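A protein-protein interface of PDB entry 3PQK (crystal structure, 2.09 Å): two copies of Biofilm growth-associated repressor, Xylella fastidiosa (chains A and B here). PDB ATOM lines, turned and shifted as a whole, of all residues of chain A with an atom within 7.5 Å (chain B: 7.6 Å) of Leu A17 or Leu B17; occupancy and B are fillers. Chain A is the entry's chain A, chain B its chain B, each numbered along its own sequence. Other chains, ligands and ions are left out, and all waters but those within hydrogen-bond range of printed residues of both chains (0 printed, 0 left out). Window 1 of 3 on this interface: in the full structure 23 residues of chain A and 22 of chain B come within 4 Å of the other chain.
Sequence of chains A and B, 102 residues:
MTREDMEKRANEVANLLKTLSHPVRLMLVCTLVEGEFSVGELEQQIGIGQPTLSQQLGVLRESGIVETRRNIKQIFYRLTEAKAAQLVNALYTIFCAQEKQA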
ATOM      1  N   ALA A  10      -0.879  10.917 -28.995  1.00  0.00           N
ATOM      2  CA  ALA A  10      -1.978   9.988 -28.755  1.00  0.00           C
ATOM      3  C   ALA A  10      -1.932   9.361 -27.351  1.00  0.00           C
ATOM      4  O   ALA A  10      -2.914   9.444 -26.621  1.00  0.00           O
ATOM      5  CB  ALA A  10      -2.008   8.915 -29.826  1.00  0.00           C
ATOM      6  N   ASN A  11      -0.785   8.778 -26.971  1.00  0.00           N
ATOM      7  CA  ASN A  11      -0.596   8.184 -25.649  1.00  0.00           C
ATOM      8  C   ASN A  11      -0.731   9.201 -24.536  1.00  0.00           C
ATOM      9  O   ASN A  11      -1.390   8.927 -23.529  1.00  0.00           O
ATOM     10  CB  ASN A  11       0.759   7.519 -25.574  1.00  0.00           C
ATOM     11  CG  ASN A  11       0.728   6.151 -26.180  1.00  0.00           C
ATOM     12  OD1 ASN A  11       0.078   5.242 -25.663  1.00  0.00           O
ATOM     13  ND2 ASN A  11       1.387   5.995 -27.313  1.00  0.00           N
ATOM     14  N   GLU A  12      -0.114  10.376 -24.730  1.00  0.00           N
ATOM     15  CA  GLU A  12      -0.131  11.474 -23.779  1.00  0.00           C
ATOM     16  C   GLU A  12      -1.576  11.928 -23.510  1.00  0.00           C
ATOM     17  O   GLU A  12      -1.974  12.070 -22.349  1.00  0.00           O
ATOM     18  CB  GLU A  12       0.737  12.648 -24.299  1.00  0.00           C
ATOM     19  CG  GLU A  12       2.235  12.389 -24.168  1.00  0.00           C
ATOM     20  CD  GLU A  12       3.199  13.419 -24.728  1.00  0.00           C
ATOM     21  OE1 GLU A  12       2.754  14.387 -25.390  1.00  0.00           O
ATOM     22  OE2 GLU A  12       4.419  13.249 -24.504  1.00  0.00           O
ATOM     23  N   VAL A  13      -2.361  12.114 -24.568  1.00  0.00           N
ATOM     24  CA  VAL A  13      -3.777  12.566 -24.475  1.00  0.00           C
ATOM     25  C   VAL A  13      -4.661  11.455 -23.860  1.00  0.00           C
ATOM     26  O   VAL A  13      -5.499  11.739 -23.005  1.00  0.00           O
ATOM     27  CB  VAL A  13      -4.289  13.094 -25.847  1.00  0.00           C
ATOM     28  CG1 VAL A  13      -5.755  13.542 -25.787  1.00  0.00           C
ATOM     29  CG2 VAL A  13      -3.425  14.255 -26.295  1.00  0.00           C
ATOM     30  N   ALA A  14      -4.410  10.189 -24.234  1.00  0.00           N
ATOM     31  CA  ALA A  14      -5.117   9.051 -23.664  1.00  0.00           C
ATOM     32  C   ALA A  14      -4.887   8.965 -22.174  1.00  0.00           C
ATOM     33  O   ALA A  14      -5.832   8.686 -21.430  1.00  0.00           O
ATOM     34  CB  ALA A  14      -4.680   7.762 -24.340  1.00  0.00           C
ATOM     35  N   ASN A  15      -3.637   9.209 -21.723  1.00  0.00           N
ATOM     36  CA  ASN A  15      -3.289   9.167 -20.292  1.00  0.00           C
ATOM     37  C   ASN A  15      -4.016  10.302 -19.552  1.00  0.00           C
ATOM     38  O   ASN A  15      -4.597  10.086 -18.485  1.00  0.00           O
ATOM     39  CB  ASN A  15      -1.758   9.240 -20.101  1.00  0.00           C
ATOM     40  CG  ASN A  15      -1.001   8.039 -20.634  1.00  0.00           C
ATOM     41  OD1 ASN A  15      -1.567   6.973 -20.906  1.00  0.00           O
ATOM     42  ND2 ASN A  15       0.297   8.203 -20.836  1.00  0.00           N
ATOM     43  N   LEU A  16      -4.070  11.485 -20.180  1.00  0.00           N
ATOM     44  CA  LEU A  16      -4.802  12.601 -19.605  1.00  0.00           C
ATOM     45  C   LEU A  16      -6.304  12.272 -19.459  1.00  0.00           C
ATOM     46  O   LEU A  16      -6.893  12.616 -18.435  1.00  0.00           O
ATOM     47  CB  LEU A  16      -4.591  13.870 -20.456  1.00  0.00           C
ATOM     48  CG  LEU A  16      -5.415  15.102 -20.037  1.00  0.00           C
ATOM     49  CD1 LEU A  16      -5.166  15.461 -18.586  1.00  0.00           C
ATOM     50  CD2 LEU A  16      -5.103  16.297 -20.923  1.00  0.00           C
ATOM     51  N   LEU A  17      -6.909  11.607 -20.474  1.00  0.00           N
ATOM     52  CA  LEU A  17      -8.338  11.235 -20.455  1.00  0.00           C
ATOM     53  C   LEU A  17      -8.597  10.189 -19.390  1.00  0.00           C
ATOM     54  O   LEU A  17      -9.641  10.240 -18.735  1.00  0.00           O
ATOM     55  CB  LEU A  17      -8.833  10.743 -21.834  1.00  0.00           C
ATOM     56  CG  LEU A  17      -8.795  11.757 -22.991  1.00  0.00           C
ATOM     57  CD1 LEU A  17      -9.307  11.135 -24.267  1.00  0.00           C
ATOM     58  CD2 LEU A  17      -9.568  13.038 -22.664  1.00  0.00           C
ATOM     59  N   LYS A  18      -7.650   9.243 -19.205  1.00  0.00           N
ATOM     60  CA  LYS A  18      -7.758   8.222 -18.145  1.00  0.00           C
ATOM     61  C   LYS A  18      -7.891   8.939 -16.800  1.00  0.00           C
ATOM     62  O   LYS A  18      -8.768   8.594 -16.010  1.00  0.00           O
ATOM     63  CB  LYS A  18      -6.515   7.314 -18.101  1.00  0.00           C
ATOM     64  CG  LYS A  18      -6.513   6.239 -19.166  1.00  0.00           C
ATOM     65  CD  LYS A  18      -5.143   5.581 -19.300  1.00  0.00           C
ATOM     66  CE  LYS A  18      -5.048   4.727 -20.542  1.00  0.00           C
ATOM     67  NZ  LYS A  18      -3.688   4.147 -20.690  1.00  0.00           N
ATOM     68  N   THR A  19      -7.047   9.971 -16.566  1.00  0.00           N
ATOM     69  CA  THR A  19      -7.055  10.743 -15.334  1.00  0.00           C
ATOM     70  C   THR A  19      -8.405  11.405 -15.104  1.00  0.00           C
ATOM     71  O   THR A  19      -8.950  11.301 -14.003  1.00  0.00           O
ATOM     72  CB  THR A  19      -5.941  11.788 -15.345  1.00  0.00           C
ATOM     73  OG1 THR A  19      -4.696  11.122 -15.515  1.00  0.00           O
ATOM     74  CG2 THR A  19      -5.939  12.647 -14.068  1.00  0.00           C
ATOM     75  N   LEU A  20      -8.947  12.061 -16.136  1.00  0.00           N
ATOM     76  CA  LEU A  20     -10.220  12.772 -16.020  1.00  0.00           C
ATOM     77  C   LEU A  20     -11.446  11.844 -16.015  1.00  0.00           C
ATOM     78  O   LEU A  20     -12.540  12.306 -15.729  1.00  0.00           O
ATOM     79  CB  LEU A  20     -10.348  13.847 -17.104  1.00  0.00           C
ATOM     80  CG  LEU A  20      -9.299  14.956 -17.110  1.00  0.00           C
ATOM     81  CD1 LEU A  20      -9.439  15.791 -18.332  1.00  0.00           C
ATOM     82  CD2 LEU A  20      -9.406  15.846 -15.861  1.00  0.00           C
ATOM     83  N   SER A  21     -11.254  10.554 -16.314  1.00  0.00           N
ATOM     84  CA  SER A  21     -12.290   9.506 -16.360  1.00  0.00           C
ATOM     85  C   SER A  21     -12.845   9.065 -14.962  1.00  0.00           C
ATOM     86  O   SER A  21     -13.014   7.864 -14.725  1.00  0.00           O
ATOM     87  CB  SER A  21     -11.750   8.276 -17.090  1.00  0.00           C
ATOM     88  OG  SER A  21     -11.880   8.469 -18.481  1.00  0.00           O
ATOM     89  N   HIS A  22     -13.127  10.022 -14.062  1.00  0.00           N
ATOM     90  CA  HIS A  22     -13.723   9.750 -12.751  1.00  0.00           C
ATOM     91  C   HIS A  22     -14.766  10.821 -12.533  1.00  0.00           C
ATOM     92  O   HIS A  22     -14.431  11.991 -12.620  1.00  0.00           O
ATOM     93  CB  HIS A  22     -12.676   9.747 -11.621  1.00  0.00           C
ATOM     94  CG  HIS A  22     -13.175   9.256 -10.290  1.00  0.00           C
ATOM     95  ND1 HIS A  22     -14.325   9.778  -9.697  1.00  0.00           N
ATOM     96  CD2 HIS A  22     -12.638   8.338  -9.453  1.00  0.00           C
ATOM     97  CE1 HIS A  22     -14.468   9.135  -8.549  1.00  0.00           C
ATOM     98  NE2 HIS A  22     -13.469   8.274  -8.347  1.00  0.00           N
ATOM     99  N   ARG A  25     -13.702  13.559 -10.102  1.00  0.00           N
ATOM    100  CA  ARG A  25     -12.664  14.419 -10.708  1.00  0.00           C
ATOM    101  C   ARG A  25     -13.280  15.392 -11.695  1.00  0.00           C
ATOM    102  O   ARG A  25     -12.923  16.564 -11.701  1.00  0.00           O
ATOM    103  CB  ARG A  25     -11.589  13.590 -11.400  1.00  0.00           C
ATOM    104  CG  ARG A  25     -10.719  12.855 -10.429  1.00  0.00           C
ATOM    105  CD  ARG A  25      -9.765  11.944 -11.155  1.00  0.00           C
ATOM    106  NE  ARG A  25      -9.410  10.790 -10.342  1.00  0.00           N
ATOM    107  CZ  ARG A  25      -8.972   9.633 -10.820  1.00  0.00           C
ATOM    108  NH1 ARG A  25      -8.829   9.458 -12.127  1.00  0.00           N
ATOM    109  NH2 ARG A  25      -8.669   8.644  -9.996  1.00  0.00           N
ATOM    110  N   LEU A  26     -14.247  14.936 -12.491  1.00  0.00           N
ATOM    111  CA  LEU A  26     -14.925  15.824 -13.426  1.00  0.00           C
ATOM    112  C   LEU A  26     -15.720  16.950 -12.751  1.00  0.00           C
ATOM    113  O   LEU A  26     -15.632  18.095 -13.183  1.00  0.00           O
ATOM    114  CB  LEU A  26     -15.795  15.035 -14.386  1.00  0.00           C
ATOM    115  CG  LEU A  26     -15.017  14.363 -15.503  1.00  0.00           C
ATOM    116  CD1 LEU A  26     -15.902  13.372 -16.247  1.00  0.00           C
ATOM    117  CD2 LEU A  26     -14.459  15.398 -16.471  1.00  0.00           C
ATOM    118  N   ILE A  65      -3.092  18.906 -12.696  1.00  0.00           N
ATOM    119  CA  ILE A  65      -4.315  19.543 -13.221  1.00  0.00           C
ATOM    120  C   ILE A  65      -4.837  20.617 -12.262  1.00  0.00           C
ATOM    121  O   ILE A  65      -5.386  21.638 -12.695  1.00  0.00           O
ATOM    122  CB  ILE A  65      -5.380  18.436 -13.554  1.00  0.00           C
ATOM    123  CG1 ILE A  65      -4.874  17.506 -14.700  1.00  0.00           C
ATOM    124  CG2 ILE A  65      -6.749  19.053 -13.935  1.00  0.00           C
ATOM    125  CD1 ILE A  65      -5.669  16.209 -14.865  1.00  0.00           C
ATOM    126  N   LEU A  87      -8.319  21.454 -21.932  1.00  0.00           N
ATOM    127  CA  LEU A  87      -9.264  20.353 -22.096  1.00  0.00           C
ATOM    128  C   LEU A  87     -10.403  20.507 -21.072  1.00  0.00           C
ATOM    129  O   LEU A  87     -11.575  20.336 -21.433  1.00  0.00           O
ATOM    130  CB  LEU A  87      -8.565  18.976 -21.959  1.00  0.00           C
ATOM    131  CG  LEU A  87      -9.504  17.726 -21.988  1.00  0.00           C
ATOM    132  CD1 LEU A  87     -10.338  17.666 -23.252  1.00  0.00           C
ATOM    133  CD2 LEU A  87      -8.700  16.435 -21.796  1.00  0.00           C
ATOM    134  N   LEU A  91     -14.414  20.707 -21.757  1.00  0.00           N
ATOM    135  CA  LEU A  91     -15.389  19.813 -21.113  1.00  0.00           C
ATOM    136  C   LEU A  91     -16.464  20.657 -20.391  1.00  0.00           C
ATOM    137  O   LEU A  91     -17.639  20.284 -20.396  1.00  0.00           O
ATOM    138  CB  LEU A  91     -14.690  18.886 -20.092  1.00  0.00           C
ATOM    139  CG  LEU A  91     -13.756  17.797 -20.644  1.00  0.00           C
ATOM    140  CD1 LEU A  91     -12.852  17.254 -19.528  1.00  0.00           C
ATOM    141  CD2 LEU A  91     -14.555  16.632 -21.286  1.00  0.00           C
ATOM    142  N   PHE A  95     -20.178  20.188 -21.740  1.00  0.00           N
ATOM    143  CA  PHE A  95     -21.028  19.440 -20.822  1.00  0.00           C
ATOM    144  C   PHE A  95     -21.548  20.148 -19.566  1.00  0.00           C
ATOM    145  O   PHE A  95     -22.762  20.212 -19.368  1.00  0.00           O
ATOM    146  CB  PHE A  95     -20.339  18.114 -20.432  1.00  0.00           C
ATOM    147  CG  PHE A  95     -19.943  17.231 -21.592  1.00  0.00           C
ATOM    148  CD1 PHE A  95     -20.884  16.419 -22.226  1.00  0.00           C
ATOM    149  CD2 PHE A  95     -18.616  17.167 -22.017  1.00  0.00           C
ATOM    150  CE1 PHE A  95     -20.518  15.581 -23.278  1.00  0.00           C
ATOM    151  CE2 PHE A  95     -18.243  16.320 -23.067  1.00  0.00           C
ATOM    152  CZ  PHE A  95     -19.199  15.532 -23.697  1.00  0.00           C
ATOM    153  N   ALA B  10     -21.805  13.910 -14.938  1.00  0.00           N
ATOM    154  CA  ALA B  10     -20.452  13.516 -14.552  1.00  0.00           C
ATOM    155  C   ALA B  10     -20.143  12.077 -14.937  1.00  0.00           C
ATOM    156  O   ALA B  10     -19.132  11.833 -15.579  1.00  0.00           O
ATOM    157  CB  ALA B  10     -20.254  13.707 -13.060  1.00  0.00           C
ATOM    158  N   ASN B  11     -21.025  11.135 -14.572  1.00  0.00           N
ATOM    159  CA  ASN B  11     -20.862   9.727 -14.895  1.00  0.00           C
ATOM    160  C   ASN B  11     -20.856   9.490 -16.400  1.00  0.00           C
ATOM    161  O   ASN B  11     -20.001   8.771 -16.910  1.00  0.00           O
ATOM    162  CB  ASN B  11     -21.951   8.907 -14.220  1.00  0.00           C
ATOM    163  CG  ASN B  11     -21.576   8.511 -12.818  1.00  0.00           C
ATOM    164  OD1 ASN B  11     -20.626   7.764 -12.592  1.00  0.00           O
ATOM    165  ND2 ASN B  11     -22.301   9.017 -11.846  1.00  0.00           N
ATOM    166  N   GLU B  12     -21.791  10.131 -17.101  1.00  0.00           N
ATOM    167  CA  GLU B  12     -21.957  10.036 -18.539  1.00  0.00           C
ATOM    168  C   GLU B  12     -20.677  10.509 -19.257  1.00  0.00           C
ATOM    169  O   GLU B  12     -20.178   9.816 -20.147  1.00  0.00           O
ATOM    170  CB  GLU B  12     -23.185  10.854 -18.982  1.00  0.00           C
ATOM    171  CG  GLU B  12     -24.523  10.194 -18.659  1.00  0.00           C
ATOM    172  CD  GLU B  12     -25.794  10.981 -18.947  1.00  0.00           C
ATOM    173  OE1 GLU B  12     -25.715  12.082 -19.538  1.00  0.00           O
ATOM    174  OE2 GLU B  12     -26.882  10.472 -18.590  1.00  0.00           O
ATOM    175  N   VAL B  13     -20.138  11.653 -18.842  1.00  0.00           N
ATOM    176  CA  VAL B  13     -18.909  12.248 -19.444  1.00  0.00           C
ATOM    177  C   VAL B  13     -17.666  11.392 -19.103  1.00  0.00           C
ATOM    178  O   VAL B  13     -16.832  11.146 -19.975  1.00  0.00           O
ATOM    179  CB  VAL B  13     -18.766  13.747 -19.064  1.00  0.00           C
ATOM    180  CG1 VAL B  13     -17.489  14.381 -19.632  1.00  0.00           C
ATOM    181  CG2 VAL B  13     -19.974  14.506 -19.566  1.00  0.00           C
ATOM    182  N   ALA B  14     -17.594  10.877 -17.865  1.00  0.00           N
ATOM    183  CA  ALA B  14     -16.508   9.996 -17.446  1.00  0.00           C
ATOM    184  C   ALA B  14     -16.498   8.736 -18.285  1.00  0.00           C
ATOM    185  O   ALA B  14     -15.421   8.280 -18.677  1.00  0.00           O
ATOM    186  CB  ALA B  14     -16.651   9.651 -15.977  1.00  0.00           C
ATOM    187  N   ASN B  15     -17.689   8.170 -18.580  1.00  0.00           N
ATOM    188  CA  ASN B  15     -17.806   6.952 -19.400  1.00  0.00           C
ATOM    189  C   ASN B  15     -17.339   7.246 -20.832  1.00  0.00           C
ATOM    190  O   ASN B  15     -16.576   6.472 -21.411  1.00  0.00           O
ATOM    191  CB  ASN B  15     -19.248   6.403 -19.366  1.00  0.00           C
ATOM    192  CG  ASN B  15     -19.697   5.905 -18.002  1.00  0.00           C
ATOM    193  OD1 ASN B  15     -18.900   5.676 -17.083  1.00  0.00           O
ATOM    194  ND2 ASN B  15     -20.997   5.761 -17.836  1.00  0.00           N
ATOM    195  N   LEU B  16     -17.713   8.428 -21.352  1.00  0.00           N
ATOM    196  CA  LEU B  16     -17.260   8.840 -22.673  1.00  0.00           C
ATOM    197  C   LEU B  16     -15.719   8.971 -22.714  1.00  0.00           C
ATOM    198  O   LEU B  16     -15.111   8.555 -23.702  1.00  0.00           O
ATOM    199  CB  LEU B  16     -17.940  10.153 -23.078  1.00  0.00           C
ATOM    200  CG  LEU B  16     -17.452  10.791 -24.394  1.00  0.00           C
ATOM    201  CD1 LEU B  16     -17.589   9.819 -25.553  1.00  0.00           C
ATOM    202  CD2 LEU B  16     -18.223  12.057 -24.709  1.00  0.00           C
ATOM    203  N   LEU B  17     -15.095   9.533 -21.646  1.00  0.00           N
ATOM    204  CA  LEU B  17     -13.635   9.719 -21.576  1.00  0.00           C
ATOM    205  C   LEU B  17     -12.938   8.373 -21.485  1.00  0.00           C
ATOM    206  O   LEU B  17     -11.879   8.200 -22.084  1.00  0.00           O
ATOM    207  CB  LEU B  17     -13.215  10.631 -20.401  1.00  0.00           C
ATOM    208  CG  LEU B  17     -13.701  12.094 -20.442  1.00  0.00           C
ATOM    209  CD1 LEU B  17     -13.227  12.855 -19.215  1.00  0.00           C
ATOM    210  CD2 LEU B  17     -13.287  12.806 -21.711  1.00  0.00           C
ATOM    211  N   LYS B  18     -13.539   7.414 -20.753  1.00  0.00           N
ATOM    212  CA  LYS B  18     -12.998   6.042 -20.655  1.00  0.00           C
ATOM    213  C   LYS B  18     -12.894   5.464 -22.073  1.00  0.00           C
ATOM    214  O   LYS B  18     -11.852   4.917 -22.437  1.00  0.00           O
ATOM    215  CB  LYS B  18     -13.908   5.133 -19.810  1.00  0.00           C
ATOM    216  CG  LYS B  18     -13.751   5.332 -18.318  1.00  0.00           C
ATOM    217  CD  LYS B  18     -14.877   4.664 -17.536  1.00  0.00           C
ATOM    218  CE  LYS B  18     -14.900   5.096 -16.088  1.00  0.00           C
ATOM    219  NZ  LYS B  18     -16.043   4.484 -15.360  1.00  0.00           N
ATOM    220  N   THR B  19     -13.957   5.640 -22.888  1.00  0.00           N
ATOM    221  CA  THR B  19     -14.003   5.156 -24.261  1.00  0.00           C
ATOM    222  C   THR B  19     -12.879   5.752 -25.098  1.00  0.00           C
ATOM    223  O   THR B  19     -12.181   5.013 -25.795  1.00  0.00           O
ATOM    224  CB  THR B  19     -15.357   5.449 -24.892  1.00  0.00           C
ATOM    225  OG1 THR B  19     -16.372   4.829 -24.100  1.00  0.00           O
ATOM    226  CG2 THR B  19     -15.428   4.975 -26.352  1.00  0.00           C
ATOM    227  N   LEU B  20     -12.698   7.079 -25.020  1.00  0.00           N
ATOM    228  CA  LEU B  20     -11.681   7.764 -25.817  1.00  0.00           C
ATOM    229  C   LEU B  20     -10.254   7.575 -25.280  1.00  0.00           C
ATOM    230  O   LEU B  20      -9.306   7.957 -25.960  1.00  0.00           O
ATOM    231  CB  LEU B  20     -12.018   9.257 -25.961  1.00  0.00           C
ATOM    232  CG  LEU B  20     -13.328   9.606 -26.660  1.00  0.00           C
ATOM    233  CD1 LEU B  20     -13.608  11.057 -26.541  1.00  0.00           C
ATOM    234  CD2 LEU B  20     -13.310   9.203 -28.149  1.00  0.00           C
ATOM    235  N   SER B  21     -10.105   6.986 -24.081  1.00  0.00           N
ATOM    236  CA  SER B  21      -8.827   6.711 -23.397  1.00  0.00           C
ATOM    237  C   SER B  21      -7.976   5.563 -24.023  1.00  0.00           C
ATOM    238  O   SER B  21      -7.423   4.738 -23.282  1.00  0.00           O
ATOM    239  CB  SER B  21      -9.082   6.406 -21.920  1.00  0.00           C
ATOM    240  OG  SER B  21      -9.212   7.620 -21.214  1.00  0.00           O
ATOM    241  N   HIS B  22      -7.857   5.526 -25.366  1.00  0.00           N
ATOM    242  CA  HIS B  22      -7.036   4.544 -26.075  1.00  0.00           C
ATOM    243  C   HIS B  22      -6.328   5.298 -27.166  1.00  0.00           C
ATOM    244  O   HIS B  22      -7.000   5.947 -27.956  1.00  0.00           O
ATOM    245  CB  HIS B  22      -7.867   3.373 -26.635  1.00  0.00           C
ATOM    246  CG  HIS B  22      -7.063   2.222 -27.181  1.00  0.00           C
ATOM    247  ND1 HIS B  22      -6.045   2.411 -28.111  1.00  0.00           N
ATOM    248  CD2 HIS B  22      -7.190   0.896 -26.944  1.00  0.00           C
ATOM    249  CE1 HIS B  22      -5.558   1.209 -28.368  1.00  0.00           C
ATOM    250  NE2 HIS B  22      -6.225   0.262 -27.704  1.00  0.00           N
ATOM    251  N   ARG B  25      -7.774   4.743 -30.654  1.00  0.00           N
ATOM    252  CA  ARG B  25      -9.092   5.397 -30.775  1.00  0.00           C
ATOM    253  C   ARG B  25      -8.933   6.891 -30.977  1.00  0.00           C
ATOM    254  O   ARG B  25      -9.604   7.465 -31.826  1.00  0.00           O
ATOM    255  CB  ARG B  25      -9.969   5.129 -29.558  1.00  0.00           C
ATOM    256  CG  ARG B  25     -10.448   3.710 -29.490  1.00  0.00           C
ATOM    257  CD  ARG B  25     -11.189   3.462 -28.197  1.00  0.00           C
ATOM    258  NE  ARG B  25     -11.086   2.068 -27.788  1.00  0.00           N
ATOM    259  CZ  ARG B  25     -11.232   1.625 -26.544  1.00  0.00           C
ATOM    260  NH1 ARG B  25     -11.491   2.471 -25.554  1.00  0.00           N
ATOM    261  NH2 ARG B  25     -11.124   0.331 -26.281  1.00  0.00           N
ATOM    262  N   LEU B  26      -8.001   7.512 -30.256  1.00  0.00           N
ATOM    263  CA  LEU B  26      -7.747   8.933 -30.433  1.00  0.00           C
ATOM    264  C   LEU B  26      -7.231   9.308 -31.831  1.00  0.00           C
ATOM    265  O   LEU B  26      -7.706  10.284 -32.409  1.00  0.00           O
ATOM    266  CB  LEU B  26      -6.823   9.467 -29.342  1.00  0.00           C
ATOM    267  CG  LEU B  26      -7.524   9.686 -28.016  1.00  0.00           C
ATOM    268  CD1 LEU B  26      -6.509   9.934 -26.904  1.00  0.00           C
ATOM    269  CD2 LEU B  26      -8.486  10.871 -28.105  1.00  0.00           C
ATOM    270  N   ILE B  65     -19.724   6.756 -31.607  1.00  0.00           N
ATOM    271  CA  ILE B  65     -18.819   7.875 -31.931  1.00  0.00           C
ATOM    272  C   ILE B  65     -18.506   7.915 -33.432  1.00  0.00           C
ATOM    273  O   ILE B  65     -18.346   8.989 -34.018  1.00  0.00           O
ATOM    274  CB  ILE B  65     -17.537   7.785 -31.030  1.00  0.00           C
ATOM    275  CG1 ILE B  65     -17.912   7.984 -29.524  1.00  0.00           C
ATOM    276  CG2 ILE B  65     -16.462   8.821 -31.445  1.00  0.00           C
ATOM    277  CD1 ILE B  65     -16.799   7.573 -28.542  1.00  0.00           C
ATOM    278  N   LEU B  87     -16.792  16.768 -28.428  1.00  0.00           N
ATOM    279  CA  LEU B  87     -15.603  16.517 -27.614  1.00  0.00           C
ATOM    280  C   LEU B  87     -14.423  16.160 -28.534  1.00  0.00           C
ATOM    281  O   LEU B  87     -13.313  16.678 -28.342  1.00  0.00           O
ATOM    282  CB  LEU B  87     -15.854  15.424 -26.556  1.00  0.00           C
ATOM    283  CG  LEU B  87     -14.610  14.969 -25.720  1.00  0.00           C
ATOM    284  CD1 LEU B  87     -13.963  16.143 -24.977  1.00  0.00           C
ATOM    285  CD2 LEU B  87     -14.979  13.853 -24.756  1.00  0.00           C
ATOM    286  N   LEU B  91     -10.776  17.966 -28.815  1.00  0.00           N
ATOM    287  CA  LEU B  91      -9.505  17.243 -28.674  1.00  0.00           C
ATOM    288  C   LEU B  91      -8.634  17.496 -29.923  1.00  0.00           C
ATOM    289  O   LEU B  91      -7.409  17.630 -29.800  1.00  0.00           O
ATOM    290  CB  LEU B  91      -9.748  15.728 -28.513  1.00  0.00           C
ATOM    291  CG  LEU B  91     -10.403  15.238 -27.213  1.00  0.00           C
ATOM    292  CD1 LEU B  91     -10.946  13.813 -27.387  1.00  0.00           C
ATOM    293  CD2 LEU B  91      -9.405  15.290 -26.015  1.00  0.00           C
ATOM    294  N   PHE B  95      -5.171  19.325 -29.226  1.00  0.00           N
ATOM    295  CA  PHE B  95      -4.017  18.440 -29.360  1.00  0.00           C
ATOM    296  C   PHE B  95      -3.556  18.050 -30.768  1.00  0.00           C
ATOM    297  O   PHE B  95      -2.397  18.296 -31.111  1.00  0.00           O
ATOM    298  CB  PHE B  95      -4.227  17.167 -28.508  1.00  0.00           C
ATOM    299  CG  PHE B  95      -4.511  17.412 -27.045  1.00  0.00           C
ATOM    300  CD1 PHE B  95      -3.475  17.704 -26.155  1.00  0.00           C
ATOM    301  CD2 PHE B  95      -5.811  17.321 -26.544  1.00  0.00           C
ATOM    302  CE1 PHE B  95      -3.730  17.932 -24.802  1.00  0.00           C
ATOM    303  CE2 PHE B  95      -6.064  17.522 -25.181  1.00  0.00           C
ATOM    304  CZ  PHE B  95      -5.019  17.824 -24.318  1.00  0.00           C
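Of the 19 printed residues of chain A, 12 touch a printed residue of chain B. Printed residues of chain A that touch a printed residue of chain B: Ala A10, Val A13, Ala A14, Leu A16, Leu A17, Lys A18, Leu A20, Ser A21, Leu A26, Leu A87, Leu A91 and Phe A95. Printed residues of chain B that touch a printed residue of chain A: Ala B10, Val B13, Ala B14, Leu B16, Leu B17, Lys B18, Leu B20, Ser B21, Leu B26, Leu B87, Leu B91 and Phe B95.
O of Leu A17 sits at hydrogen-bond distance from OG of Ser A21. The side-chain hydroxyl of Ser B21 sits at hydrogen-bond distance from the backbone carbonyl oxygen of Leu B17, at 2.9 Å.
Asn A11 touches none of the printed residues of chain B. Of the printed residues of chain B, Val A13 touches Leu B26 (3.9 Å) and Phe B95 (3.4 Å). Printed residues of chain B within 4 Å of Leu A16: Phe B95 (3.7 Å). Leu A17 touches just these residues of chain B: Leu B17 (3.8 Å), Leu B20 (3.6 Å), Ser B21 (3.2 Å) and Leu B26 (3.9 Å). Ile A65 touches none of the printed residues of chain B. Printed residues of chain A within 4 Å of Leu B17: Leu A17, Leu A20, Ser A21 and Leu A26. Of the printed residues of chain A, Leu B26 touches Ala A10 (3.6 Å), Val A13 (3.9 Å), Ala A14 (3.4 Å) and Leu A17 (3.9 Å). The nearest residue of chain B that does not touch Leu A17 is Leu B91 (4.04 Å). The nearest residue of chain A that does not touch Leu B17 is Leu A91 (4.1 Å).
The backbone NH (N) of Lys A18 lies within hydrogen-bond range of the side-chain hydroxyl (OG) of Ser B21 (3.0 Å). The backbone NH (N) of Lys B18 lies within hydrogen-bond range of the side-chain hydroxyl (OG) of Ser A21, at 3.0 Å.
O of Ala A10 touches CD1 of Leu B26, at 3.6 Å. Val A13 touches Leu B26 (CG1 to CD1, 3.9 Å). Phe B95 touches Val A13. Leu B26 touches Ala A14 (CD1 to N, 3.4 Å). CD2 of Leu B17 touches CD2 of Leu A17, at 3.8 Å. Ser B21 touches Leu A17. Ser A21 touches Ser B21. Leu A26 touches Val B13. CD1 of Leu A26 touches N of Ala B14, 3.4 Å away. CZ of Phe A95 touches CD2 of Leu B16, 3.7 Å away.
Ala A10 touches Leu B26, and with the chains exchanged Leu A26 touches Ala B10. Ala A14 touches Leu B26, and with the chains exchanged Leu A26 touches Ala B14. Leu A17 touches Ser B21, and with the chains exchanged Ser A21 touches Leu B17. Lys A18 touches Ser B21, and with the chains exchanged Ser A21 touches Lys B18. Positions printed for both chains: 10, 11, 12, 13, 14, 15, 16, 17, 18, 19, 20, 21, 22, 25, 26, 65, 87, 91 and 95. Of the 24 pairs that touch across the chains among the printed residues, 24 have their exchanged pair printed and touching as well.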
